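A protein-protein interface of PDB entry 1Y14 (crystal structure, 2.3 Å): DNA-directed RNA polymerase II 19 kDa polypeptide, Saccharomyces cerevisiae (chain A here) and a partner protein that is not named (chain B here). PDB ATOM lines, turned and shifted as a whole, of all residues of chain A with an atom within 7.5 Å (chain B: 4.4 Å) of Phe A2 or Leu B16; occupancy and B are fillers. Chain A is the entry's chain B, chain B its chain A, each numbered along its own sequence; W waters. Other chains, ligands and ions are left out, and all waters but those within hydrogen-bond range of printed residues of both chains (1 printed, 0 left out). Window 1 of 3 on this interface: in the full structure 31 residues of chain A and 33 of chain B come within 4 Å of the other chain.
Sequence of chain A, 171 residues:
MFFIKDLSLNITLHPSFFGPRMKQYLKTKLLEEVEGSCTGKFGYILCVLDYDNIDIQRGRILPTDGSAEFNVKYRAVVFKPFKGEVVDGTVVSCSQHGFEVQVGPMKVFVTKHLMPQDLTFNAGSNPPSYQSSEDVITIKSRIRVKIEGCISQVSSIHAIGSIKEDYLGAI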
ATOM      1  N   MET A   1      19.743 -22.716  -8.936  1.00  0.00           N
ATOM      2  CA  MET A   1      18.833 -21.547  -9.058  1.00  0.00           C
ATOM      3  C   MET A   1      18.037 -21.621 -10.351  1.00  0.00           C
ATOM      4  O   MET A   1      18.509 -22.170 -11.347  1.00  0.00           O
ATOM      5  CB  MET A   1      19.633 -20.231  -9.024  1.00  0.00           C
ATOM      6  CG  MET A   1      18.743 -19.008  -8.839  1.00  0.00           C
ATOM      7  SD  MET A   1      19.657 -17.503  -8.457  1.00  0.00           S
ATOM      8  CE  MET A   1      19.746 -17.625  -6.647  1.00  0.00           C
ATOM      9  N   PHE A   2      16.824 -21.076 -10.323  1.00  0.00           N
ATOM     10  CA  PHE A   2      15.972 -21.057 -11.511  1.00  0.00           C
ATOM     11  C   PHE A   2      16.047 -19.692 -12.162  1.00  0.00           C
ATOM     12  O   PHE A   2      16.075 -18.669 -11.469  1.00  0.00           O
ATOM     13  CB  PHE A   2      14.505 -21.335 -11.163  1.00  0.00           C
ATOM     14  CG  PHE A   2      14.253 -22.709 -10.612  1.00  0.00           C
ATOM     15  CD1 PHE A   2      14.428 -22.973  -9.256  1.00  0.00           C
ATOM     16  CD2 PHE A   2      13.871 -23.750 -11.453  1.00  0.00           C
ATOM     17  CE1 PHE A   2      14.227 -24.263  -8.742  1.00  0.00           C
ATOM     18  CE2 PHE A   2      13.668 -25.035 -10.955  1.00  0.00           C
ATOM     19  CZ  PHE A   2      13.846 -25.294  -9.594  1.00  0.00           C
ATOM     20  N   PHE A   3      16.087 -19.679 -13.491  1.00  0.00           N
ATOM     21  CA  PHE A   3      16.112 -18.433 -14.252  1.00  0.00           C
ATOM     22  C   PHE A   3      15.197 -18.566 -15.457  1.00  0.00           C
ATOM     23  O   PHE A   3      14.729 -19.656 -15.786  1.00  0.00           O
ATOM     24  CB  PHE A   3      17.504 -18.131 -14.812  1.00  0.00           C
ATOM     25  CG  PHE A   3      18.608 -18.276 -13.827  1.00  0.00           C
ATOM     26  CD1 PHE A   3      19.202 -19.517 -13.605  1.00  0.00           C
ATOM     27  CD2 PHE A   3      19.076 -17.166 -13.126  1.00  0.00           C
ATOM     28  CE1 PHE A   3      20.254 -19.650 -12.695  1.00  0.00           C
ATOM     29  CE2 PHE A   3      20.123 -17.284 -12.215  1.00  0.00           C
ATOM     30  CZ  PHE A   3      20.716 -18.528 -11.995  1.00  0.00           C
ATOM     31  N   ILE A   4      14.942 -17.438 -16.109  1.00  0.00           N
ATOM     32  CA  ILE A   4      14.183 -17.425 -17.354  1.00  0.00           C
ATOM     33  C   ILE A   4      15.291 -16.940 -18.270  1.00  0.00           C
ATOM     34  O   ILE A   4      15.852 -15.871 -18.042  1.00  0.00           O
ATOM     35  CB  ILE A   4      13.047 -16.391 -17.378  1.00  0.00           C
ATOM     36  CG1 ILE A   4      11.942 -16.793 -16.400  1.00  0.00           C
ATOM     37  CG2 ILE A   4      12.491 -16.284 -18.788  1.00  0.00           C
ATOM     38  CD1 ILE A   4      10.769 -15.816 -16.379  1.00  0.00           C
ATOM     39  N   LYS A   5      15.630 -17.716 -19.286  1.00  0.00           N
ATOM     40  CA  LYS A   5      16.712 -17.327 -20.172  1.00  0.00           C
ATOM     41  C   LYS A   5      16.302 -17.322 -21.652  1.00  0.00           C
ATOM     42  O   LYS A   5      15.532 -18.183 -22.104  1.00  0.00           O
ATOM     43  CB  LYS A   5      17.901 -18.272 -19.909  1.00  0.00           C
ATOM     44  CG  LYS A   5      19.117 -18.138 -20.819  1.00  0.00           C
ATOM     45  CD  LYS A   5      19.659 -16.718 -20.872  1.00  0.00           C
ATOM     46  CE  LYS A   5      20.836 -16.622 -21.849  1.00  0.00           C
ATOM     47  NZ  LYS A   5      21.131 -15.213 -22.254  1.00  0.00           N
ATOM     48  N   TYR A  44      19.806 -27.071 -16.831  1.00  0.00           N
ATOM     49  CA  TYR A  44      18.654 -27.807 -17.327  1.00  0.00           C
ATOM     50  C   TYR A  44      17.638 -26.891 -18.029  1.00  0.00           C
ATOM     51  O   TYR A  44      17.177 -25.904 -17.449  1.00  0.00           O
ATOM     52  CB  TYR A  44      17.938 -28.525 -16.184  1.00  0.00           C
ATOM     53  CG  TYR A  44      18.721 -29.594 -15.470  1.00  0.00           C
ATOM     54  CD1 TYR A  44      19.684 -29.267 -14.509  1.00  0.00           C
ATOM     55  CD2 TYR A  44      18.444 -30.940 -15.691  1.00  0.00           C
ATOM     56  CE1 TYR A  44      20.332 -30.256 -13.778  1.00  0.00           C
ATOM     57  CE2 TYR A  44      19.090 -31.939 -14.964  1.00  0.00           C
ATOM     58  CZ  TYR A  44      20.027 -31.589 -14.008  1.00  0.00           C
ATOM     59  OH  TYR A  44      20.618 -32.570 -13.253  1.00  0.00           O
ATOM     60  N   LEU A  46      14.339 -26.813 -18.666  1.00  0.00           N
ATOM     61  CA  LEU A  46      13.147 -27.489 -18.182  1.00  0.00           C
ATOM     62  C   LEU A  46      11.813 -27.266 -18.888  1.00  0.00           C
ATOM     63  O   LEU A  46      11.041 -28.205 -19.065  1.00  0.00           O
ATOM     64  CB  LEU A  46      12.978 -27.160 -16.696  1.00  0.00           C
ATOM     65  CG  LEU A  46      14.140 -27.567 -15.788  1.00  0.00           C
ATOM     66  CD1 LEU A  46      14.050 -26.814 -14.473  1.00  0.00           C
ATOM     67  CD2 LEU A  46      14.108 -29.075 -15.551  1.00  0.00           C
ATOM     68  N   LEU A  49       8.762 -21.529 -22.704  1.00  0.00           N
ATOM     69  CA  LEU A  49       7.629 -20.676 -22.366  1.00  0.00           C
ATOM     70  C   LEU A  49       6.995 -19.983 -23.553  1.00  0.00           C
ATOM     71  O   LEU A  49       7.547 -19.967 -24.656  1.00  0.00           O
ATOM     72  CB  LEU A  49       8.081 -19.582 -21.398  1.00  0.00           C
ATOM     73  CG  LEU A  49       8.936 -19.988 -20.208  1.00  0.00           C
ATOM     74  CD1 LEU A  49       9.372 -18.735 -19.484  1.00  0.00           C
ATOM     75  CD2 LEU A  49       8.148 -20.913 -19.285  1.00  0.00           C
ATOM     76  N   ALA A  76      12.868 -19.742 -21.902  1.00  0.00           N
ATOM     77  CA  ALA A  76      12.652 -20.965 -21.142  1.00  0.00           C
ATOM     78  C   ALA A  76      13.052 -20.847 -19.681  1.00  0.00           C
ATOM     79  O   ALA A  76      13.866 -20.000 -19.314  1.00  0.00           O
ATOM     80  CB  ALA A  76      13.445 -22.098 -21.786  1.00  0.00           C
ATOM     81  N   VAL A  77      12.482 -21.707 -18.846  1.00  0.00           N
ATOM     82  CA  VAL A  77      12.859 -21.731 -17.435  1.00  0.00           C
ATOM     83  C   VAL A  77      14.040 -22.712 -17.354  1.00  0.00           C
ATOM     84  O   VAL A  77      13.888 -23.895 -17.660  1.00  0.00           O
ATOM     85  CB  VAL A  77      11.722 -22.266 -16.546  1.00  0.00           C
ATOM     86  CG1 VAL A  77      12.265 -22.639 -15.161  1.00  0.00           C
ATOM     87  CG2 VAL A  77      10.623 -21.218 -16.415  1.00  0.00           C
ATOM     88  N   VAL A  78      15.216 -22.225 -16.974  1.00  0.00           N
ATOM     89  CA  VAL A  78      16.372 -23.113 -16.851  1.00  0.00           C
ATOM     90  C   VAL A  78      16.805 -23.187 -15.395  1.00  0.00           C
ATOM     91  O   VAL A  78      16.542 -22.272 -14.612  1.00  0.00           O
ATOM     92  CB  VAL A  78      17.578 -22.627 -17.675  1.00  0.00           C
ATOM     93  CG1 VAL A  78      17.128 -22.185 -19.061  1.00  0.00           C
ATOM     94  CG2 VAL A  78      18.299 -21.514 -16.940  1.00  0.00           C
ATOM     95  N   PHE A  79      17.462 -24.282 -15.029  1.00  0.00           N
ATOM     96  CA  PHE A  79      17.933 -24.438 -13.668  1.00  0.00           C
ATOM     97  C   PHE A  79      19.421 -24.746 -13.709  1.00  0.00           C
ATOM     98  O   PHE A  79      19.866 -25.586 -14.489  1.00  0.00           O
ATOM     99  CB  PHE A  79      17.197 -25.569 -12.956  1.00  0.00           C
ATOM    100  CG  PHE A  79      17.754 -25.885 -11.590  1.00  0.00           C
ATOM    101  CD1 PHE A  79      17.213 -25.294 -10.440  1.00  0.00           C
ATOM    102  CD2 PHE A  79      18.843 -26.752 -11.455  1.00  0.00           C
ATOM    103  CE1 PHE A  79      17.750 -25.563  -9.174  1.00  0.00           C
ATOM    104  CE2 PHE A  79      19.391 -27.030 -10.199  1.00  0.00           C
ATOM    105  CZ  PHE A  79      18.846 -26.437  -9.052  1.00  0.00           C
ATOM    106  N   LYS A  80      20.189 -24.041 -12.884  1.00  0.00           N
ATOM    107  CA  LYS A  80      21.633 -24.252 -12.803  1.00  0.00           C
ATOM    108  C   LYS A  80      22.110 -23.861 -11.426  1.00  0.00           C
ATOM    109  O   LYS A  80      21.924 -22.724 -10.982  1.00  0.00           O
ATOM    110  CB  LYS A  80      22.384 -23.417 -13.832  1.00  0.00           C
ATOM    111  CG  LYS A  80      23.846 -23.836 -13.994  1.00  0.00           C
ATOM    112  CD  LYS A  80      24.611 -22.833 -14.850  1.00  0.00           C
ATOM    113  CE  LYS A  80      26.087 -23.192 -14.957  1.00  0.00           C
ATOM    114  NZ  LYS A  80      26.303 -24.426 -15.758  1.00  0.00           N
ATOM    115  N   PRO A  81      22.732 -24.805 -10.721  1.00  0.00           N
ATOM    116  CA  PRO A  81      23.236 -24.537  -9.374  1.00  0.00           C
ATOM    117  C   PRO A  81      24.494 -23.673  -9.429  1.00  0.00           C
ATOM    118  O   PRO A  81      25.259 -23.738 -10.398  1.00  0.00           O
ATOM    119  CB  PRO A  81      23.508 -25.936  -8.844  1.00  0.00           C
ATOM    120  CG  PRO A  81      23.998 -26.645 -10.070  1.00  0.00           C
ATOM    121  CD  PRO A  81      23.023 -26.192 -11.131  1.00  0.00           C
ATOM    122  N   PHE A  82      24.676 -22.837  -8.414  1.00  0.00           N
ATOM    123  CA  PHE A  82      25.850 -21.975  -8.330  1.00  0.00           C
ATOM    124  C   PHE A  82      26.535 -22.204  -6.994  1.00  0.00           C
ATOM    125  O   PHE A  82      25.869 -22.367  -5.964  1.00  0.00           O
ATOM    126  CB  PHE A  82      25.471 -20.488  -8.472  1.00  0.00           C
ATOM    127  CG  PHE A  82      25.233 -20.058  -9.897  1.00  0.00           C
ATOM    128  CD1 PHE A  82      24.161 -20.569 -10.629  1.00  0.00           C
ATOM    129  CD2 PHE A  82      26.102 -19.167 -10.523  1.00  0.00           C
ATOM    130  CE1 PHE A  82      23.960 -20.199 -11.972  1.00  0.00           C
ATOM    131  CE2 PHE A  82      25.910 -18.790 -11.864  1.00  0.00           C
ATOM    132  CZ  PHE A  82      24.838 -19.308 -12.587  1.00  0.00           C
ATOM    133  N   GLU A  85      25.454 -21.242  -3.261  1.00  0.00           N
ATOM    134  CA  GLU A  85      24.008 -21.123  -3.118  1.00  0.00           C
ATOM    135  C   GLU A  85      23.487 -22.070  -2.031  1.00  0.00           C
ATOM    136  O   GLU A  85      23.934 -23.212  -1.920  1.00  0.00           O
ATOM    137  CB  GLU A  85      23.313 -21.396  -4.467  1.00  0.00           C
ATOM    138  CG  GLU A  85      21.828 -21.751  -4.357  1.00  0.00           C
ATOM    139  CD  GLU A  85      21.117 -21.916  -5.706  1.00  0.00           C
ATOM    140  OE1 GLU A  85      21.739 -22.417  -6.668  1.00  0.00           O
ATOM    141  OE2 GLU A  85      19.916 -21.560  -5.796  1.00  0.00           O
ATOM    142  N   VAL A 103      17.005 -31.626  -5.313  1.00  0.00           N
ATOM    143  CA  VAL A 103      16.804 -30.179  -5.400  1.00  0.00           C
ATOM    144  C   VAL A 103      16.390 -29.890  -6.839  1.00  0.00           C
ATOM    145  O   VAL A 103      17.225 -29.914  -7.749  1.00  0.00           O
ATOM    146  CB  VAL A 103      18.102 -29.383  -5.109  1.00  0.00           C
ATOM    147  CG1 VAL A 103      17.863 -27.901  -5.373  1.00  0.00           C
ATOM    148  CG2 VAL A 103      18.549 -29.603  -3.662  1.00  0.00           C
ATOM    149  N   GLY A 104      15.106 -29.624  -7.055  1.00  0.00           N
ATOM    150  CA  GLY A 104      14.656 -29.362  -8.411  1.00  0.00           C
ATOM    151  C   GLY A 104      14.867 -30.602  -9.268  1.00  0.00           C
ATOM    152  O   GLY A 104      14.542 -31.703  -8.844  1.00  0.00           O
ATOM    153  N   PRO A 105      15.424 -30.460 -10.474  1.00  0.00           N
ATOM    154  CA  PRO A 105      15.669 -31.581 -11.386  1.00  0.00           C
ATOM    155  C   PRO A 105      16.972 -32.302 -11.052  1.00  0.00           C
ATOM    156  O   PRO A 105      17.388 -33.225 -11.766  1.00  0.00           O
ATOM    157  CB  PRO A 105      15.786 -30.887 -12.736  1.00  0.00           C
ATOM    158  CG  PRO A 105      16.575 -29.636 -12.350  1.00  0.00           C
ATOM    159  CD  PRO A 105      15.855 -29.182 -11.077  1.00  0.00           C
ATOM    160  N   ILE B  14      17.209 -13.802 -15.789  1.00  0.00           N
ATOM    161  CA  ILE B  14      16.157 -13.345 -14.889  1.00  0.00           C
ATOM    162  C   ILE B  14      16.011 -14.429 -13.823  1.00  0.00           C
ATOM    163  O   ILE B  14      15.605 -15.547 -14.123  1.00  0.00           O
ATOM    164  CB  ILE B  14      14.818 -13.165 -15.639  1.00  0.00           C
ATOM    165  CG1 ILE B  14      14.968 -12.101 -16.733  1.00  0.00           C
ATOM    166  CG2 ILE B  14      13.740 -12.767 -14.670  1.00  0.00           C
ATOM    167  CD1 ILE B  14      13.660 -11.735 -17.455  1.00  0.00           C
ATOM    168  N   ALA B  15      16.358 -14.095 -12.586  1.00  0.00           N
ATOM    169  CA  ALA B  15      16.295 -15.043 -11.483  1.00  0.00           C
ATOM    170  C   ALA B  15      14.903 -15.108 -10.897  1.00  0.00           C
ATOM    171  O   ALA B  15      14.250 -14.088 -10.732  1.00  0.00           O
ATOM    172  CB  ALA B  15      17.302 -14.654 -10.398  1.00  0.00           C
ATOM    173  N   LEU B  16      14.447 -16.316 -10.573  1.00  0.00           N
ATOM    174  CA  LEU B  16      13.113 -16.489 -10.002  1.00  0.00           C
ATOM    175  C   LEU B  16      13.200 -17.164  -8.650  1.00  0.00           C
ATOM    176  O   LEU B  16      14.075 -18.001  -8.448  1.00  0.00           O
ATOM    177  CB  LEU B  16      12.262 -17.393 -10.895  1.00  0.00           C
ATOM    178  CG  LEU B  16      12.169 -17.135 -12.394  1.00  0.00           C
ATOM    179  CD1 LEU B  16      11.703 -18.399 -13.097  1.00  0.00           C
ATOM    180  CD2 LEU B  16      11.213 -15.983 -12.640  1.00  0.00           C
ATOM    181  N   ASN B  17      12.320 -16.798  -7.718  1.00  0.00           N
ATOM    182  CA  ASN B  17      12.302 -17.511  -6.456  1.00  0.00           C
ATOM    183  C   ASN B  17      11.483 -18.777  -6.809  1.00  0.00           C
ATOM    184  O   ASN B  17      10.894 -18.863  -7.886  1.00  0.00           O
ATOM    185  CB  ASN B  17      11.655 -16.685  -5.319  1.00  0.00           C
ATOM    186  CG  ASN B  17      10.196 -16.279  -5.600  1.00  0.00           C
ATOM    187  OD1 ASN B  17       9.373 -17.095  -5.982  1.00  0.00           O
ATOM    188  ND2 ASN B  17       9.878 -15.005  -5.368  1.00  0.00           N
ATOM    189  N   LEU B  18      11.459 -19.763  -5.929  1.00  0.00           N
ATOM    190  CA  LEU B  18      10.734 -20.995  -6.222  1.00  0.00           C
ATOM    191  C   LEU B  18       9.279 -20.765  -6.616  1.00  0.00           C
ATOM    192  O   LEU B  18       8.801 -21.319  -7.607  1.00  0.00           O
ATOM    193  CB  LEU B  18      10.811 -21.938  -5.011  1.00  0.00           C
ATOM    194  CG  LEU B  18      11.899 -23.026  -4.957  1.00  0.00           C
ATOM    195  CD1 LEU B  18      13.118 -22.664  -5.807  1.00  0.00           C
ATOM    196  CD2 LEU B  18      12.277 -23.265  -3.511  1.00  0.00           C
ATOM    197  N   GLU B  20       7.762 -18.218  -7.964  1.00  0.00           N
ATOM    198  CA  GLU B  20       7.522 -17.627  -9.276  1.00  0.00           C
ATOM    199  C   GLU B  20       7.790 -18.654 -10.375  1.00  0.00           C
ATOM    200  O   GLU B  20       7.127 -18.644 -11.408  1.00  0.00           O
ATOM    201  CB  GLU B  20       8.435 -16.427  -9.531  1.00  0.00           C
ATOM    202  CG  GLU B  20       8.408 -15.346  -8.487  1.00  0.00           C
ATOM    203  CD  GLU B  20       9.491 -14.315  -8.738  1.00  0.00           C
ATOM    204  OE1 GLU B  20      10.678 -14.665  -8.604  1.00  0.00           O
ATOM    205  OE2 GLU B  20       9.156 -13.162  -9.082  1.00  0.00           O
ATOM    206  N   ALA B  21       8.787 -19.516 -10.168  1.00  0.00           N
ATOM    207  CA  ALA B  21       9.127 -20.533 -11.165  1.00  0.00           C
ATOM    208  C   ALA B  21       7.936 -21.472 -11.296  1.00  0.00           C
ATOM    209  O   ALA B  21       7.565 -21.872 -12.398  1.00  0.00           O
ATOM    210  CB  ALA B  21      10.380 -21.300 -10.733  1.00  0.00           C
ATOM    211  N   THR B 110      11.035 -31.436 -11.081  1.00  0.00           N
ATOM    212  CA  THR B 110      10.978 -30.011 -10.772  1.00  0.00           C
ATOM    213  C   THR B 110       9.616 -29.584 -10.230  1.00  0.00           C
ATOM    214  O   THR B 110       9.517 -28.936  -9.175  1.00  0.00           O
ATOM    215  CB  THR B 110      11.298 -29.190 -12.020  1.00  0.00           C
ATOM    216  OG1 THR B 110      12.673 -29.410 -12.372  1.00  0.00           O
ATOM    217  CG2 THR B 110      11.017 -27.706 -11.779  1.00  0.00           C
ATOM    218  N   TYR B 113       8.939 -30.795  -6.800  1.00  0.00           N
ATOM    219  CA  TYR B 113       9.786 -30.007  -5.912  1.00  0.00           C
ATOM    220  C   TYR B 113       9.125 -28.644  -5.667  1.00  0.00           C
ATOM    221  O   TYR B 113       8.870 -28.251  -4.526  1.00  0.00           O
ATOM    222  CB  TYR B 113      11.165 -29.807  -6.572  1.00  0.00           C
ATOM    223  CG  TYR B 113      12.098 -28.906  -5.792  1.00  0.00           C
ATOM    224  CD1 TYR B 113      12.627 -29.310  -4.556  1.00  0.00           C
ATOM    225  CD2 TYR B 113      12.453 -27.644  -6.286  1.00  0.00           C
ATOM    226  CE1 TYR B 113      13.494 -28.472  -3.830  1.00  0.00           C
ATOM    227  CE2 TYR B 113      13.320 -26.798  -5.569  1.00  0.00           C
ATOM    228  CZ  TYR B 113      13.832 -27.216  -4.347  1.00  0.00           C
ATOM    229  OH  TYR B 113      14.667 -26.377  -3.646  1.00  0.00           O
ATOM    230  N   LEU B 114       8.851 -27.930  -6.753  1.00  0.00           N
ATOM    231  CA  LEU B 114       8.215 -26.617  -6.655  1.00  0.00           C
ATOM    232  C   LEU B 114       6.890 -26.709  -5.890  1.00  0.00           C
ATOM    233  O   LEU B 114       6.555 -25.833  -5.084  1.00  0.00           O
ATOM    234  CB  LEU B 114       8.010 -26.027  -8.064  1.00  0.00           C
ATOM    235  CG  LEU B 114       9.342 -25.744  -8.786  1.00  0.00           C
ATOM    236  CD1 LEU B 114       9.088 -25.163 -10.162  1.00  0.00           C
ATOM    237  CD2 LEU B 114      10.188 -24.774  -7.949  1.00  0.00           C
ATOM    238  N   ALA B 144      16.039 -13.436  -5.284  1.00  0.00           N
ATOM    239  CA  ALA B 144      15.561 -14.788  -5.566  1.00  0.00           C
ATOM    240  C   ALA B 144      15.780 -15.695  -4.368  1.00  0.00           C
ATOM    241  O   ALA B 144      14.939 -16.534  -4.060  1.00  0.00           O
ATOM    242  CB  ALA B 144      16.276 -15.373  -6.792  1.00  0.00           C
HETATM  243  O   HOH W   1      15.668 -20.087  -7.706  1.00  0.00           O
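The backbone NH (N) of Ile A4 is in hydrogen-bond range of the backbone carbonyl oxygen (O) of Ile B14 (2.8 Å).
The backbone carbonyl oxygen (O) of Phe A2 lies within hydrogen-bond range of the backbone NH (N) of Leu B16, at 3.0 Å.
The backbone carbonyl oxygen of Val A78 sits at hydrogen-bond distance from the backbone NH of Phe A3 (2.9 Å).
The backbone NH of Leu A46 lies within hydrogen-bond range of the backbone carbonyl oxygen of Val A77.
Among the printed residues, pairs that only touch across the chains: Phe A2 with Ala B15, Phe A2 with Leu B18, Phe A2 with Thr B110, Phe A3 with Ile B14, Phe A3 with Ala B15, Ile A4 with Leu B16, Leu A46 with Thr B110, Val A103 with Tyr B113, Gly A104 with Thr B110, Gly A104 with Tyr B113 and Pro A105 with Thr B110.
Phe A2 touches just these residues of chain B: Ala B15, Leu B16, Leu B18 and Thr B110.
Printed residues of chain A within 4 Å of Ile B14: Phe A3 (2.9 Å) and Ile A4 (2.8 Å).
Of the printed residues of chain A, Leu B18 touches Phe A2.
Printed residues of chain B within 4 Å of Val A103: Tyr B113 (3.9 Å).
The nearest residue of chain B that does not touch Phe A2 is Leu B114 (4.04 Å).
The nearest printed residue of chain A that does not touch Leu B18 is Phe A79 (6.4 Å).
Hydrophobic or aromatic side chains of chain B that line the printed part of chain A: Ile B14, Leu B16, Leu B18 and Tyr B113.
Of the 19 printed residues of chain A, 7 touch a printed residue of chain B.
Printed residues of chain A that touch a printed residue of chain B: Phe A2, Phe A3, Ile A4, Leu A46, Val A103, Gly A104 and Pro A105.
Hydrophobic or aromatic side chains of chain A that line the printed part of chain B: Phe A2, Phe A3, Ile A4, Leu A46, Val A103 and Pro A105.
Among the printed residues, no Asp or Glu carboxylate lies within 4 Å of a Lys or Arg side-chain nitrogen of the other chain.
Water W1 lies within hydrogen-bond range of O of Leu B16 and N of Phe A2.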
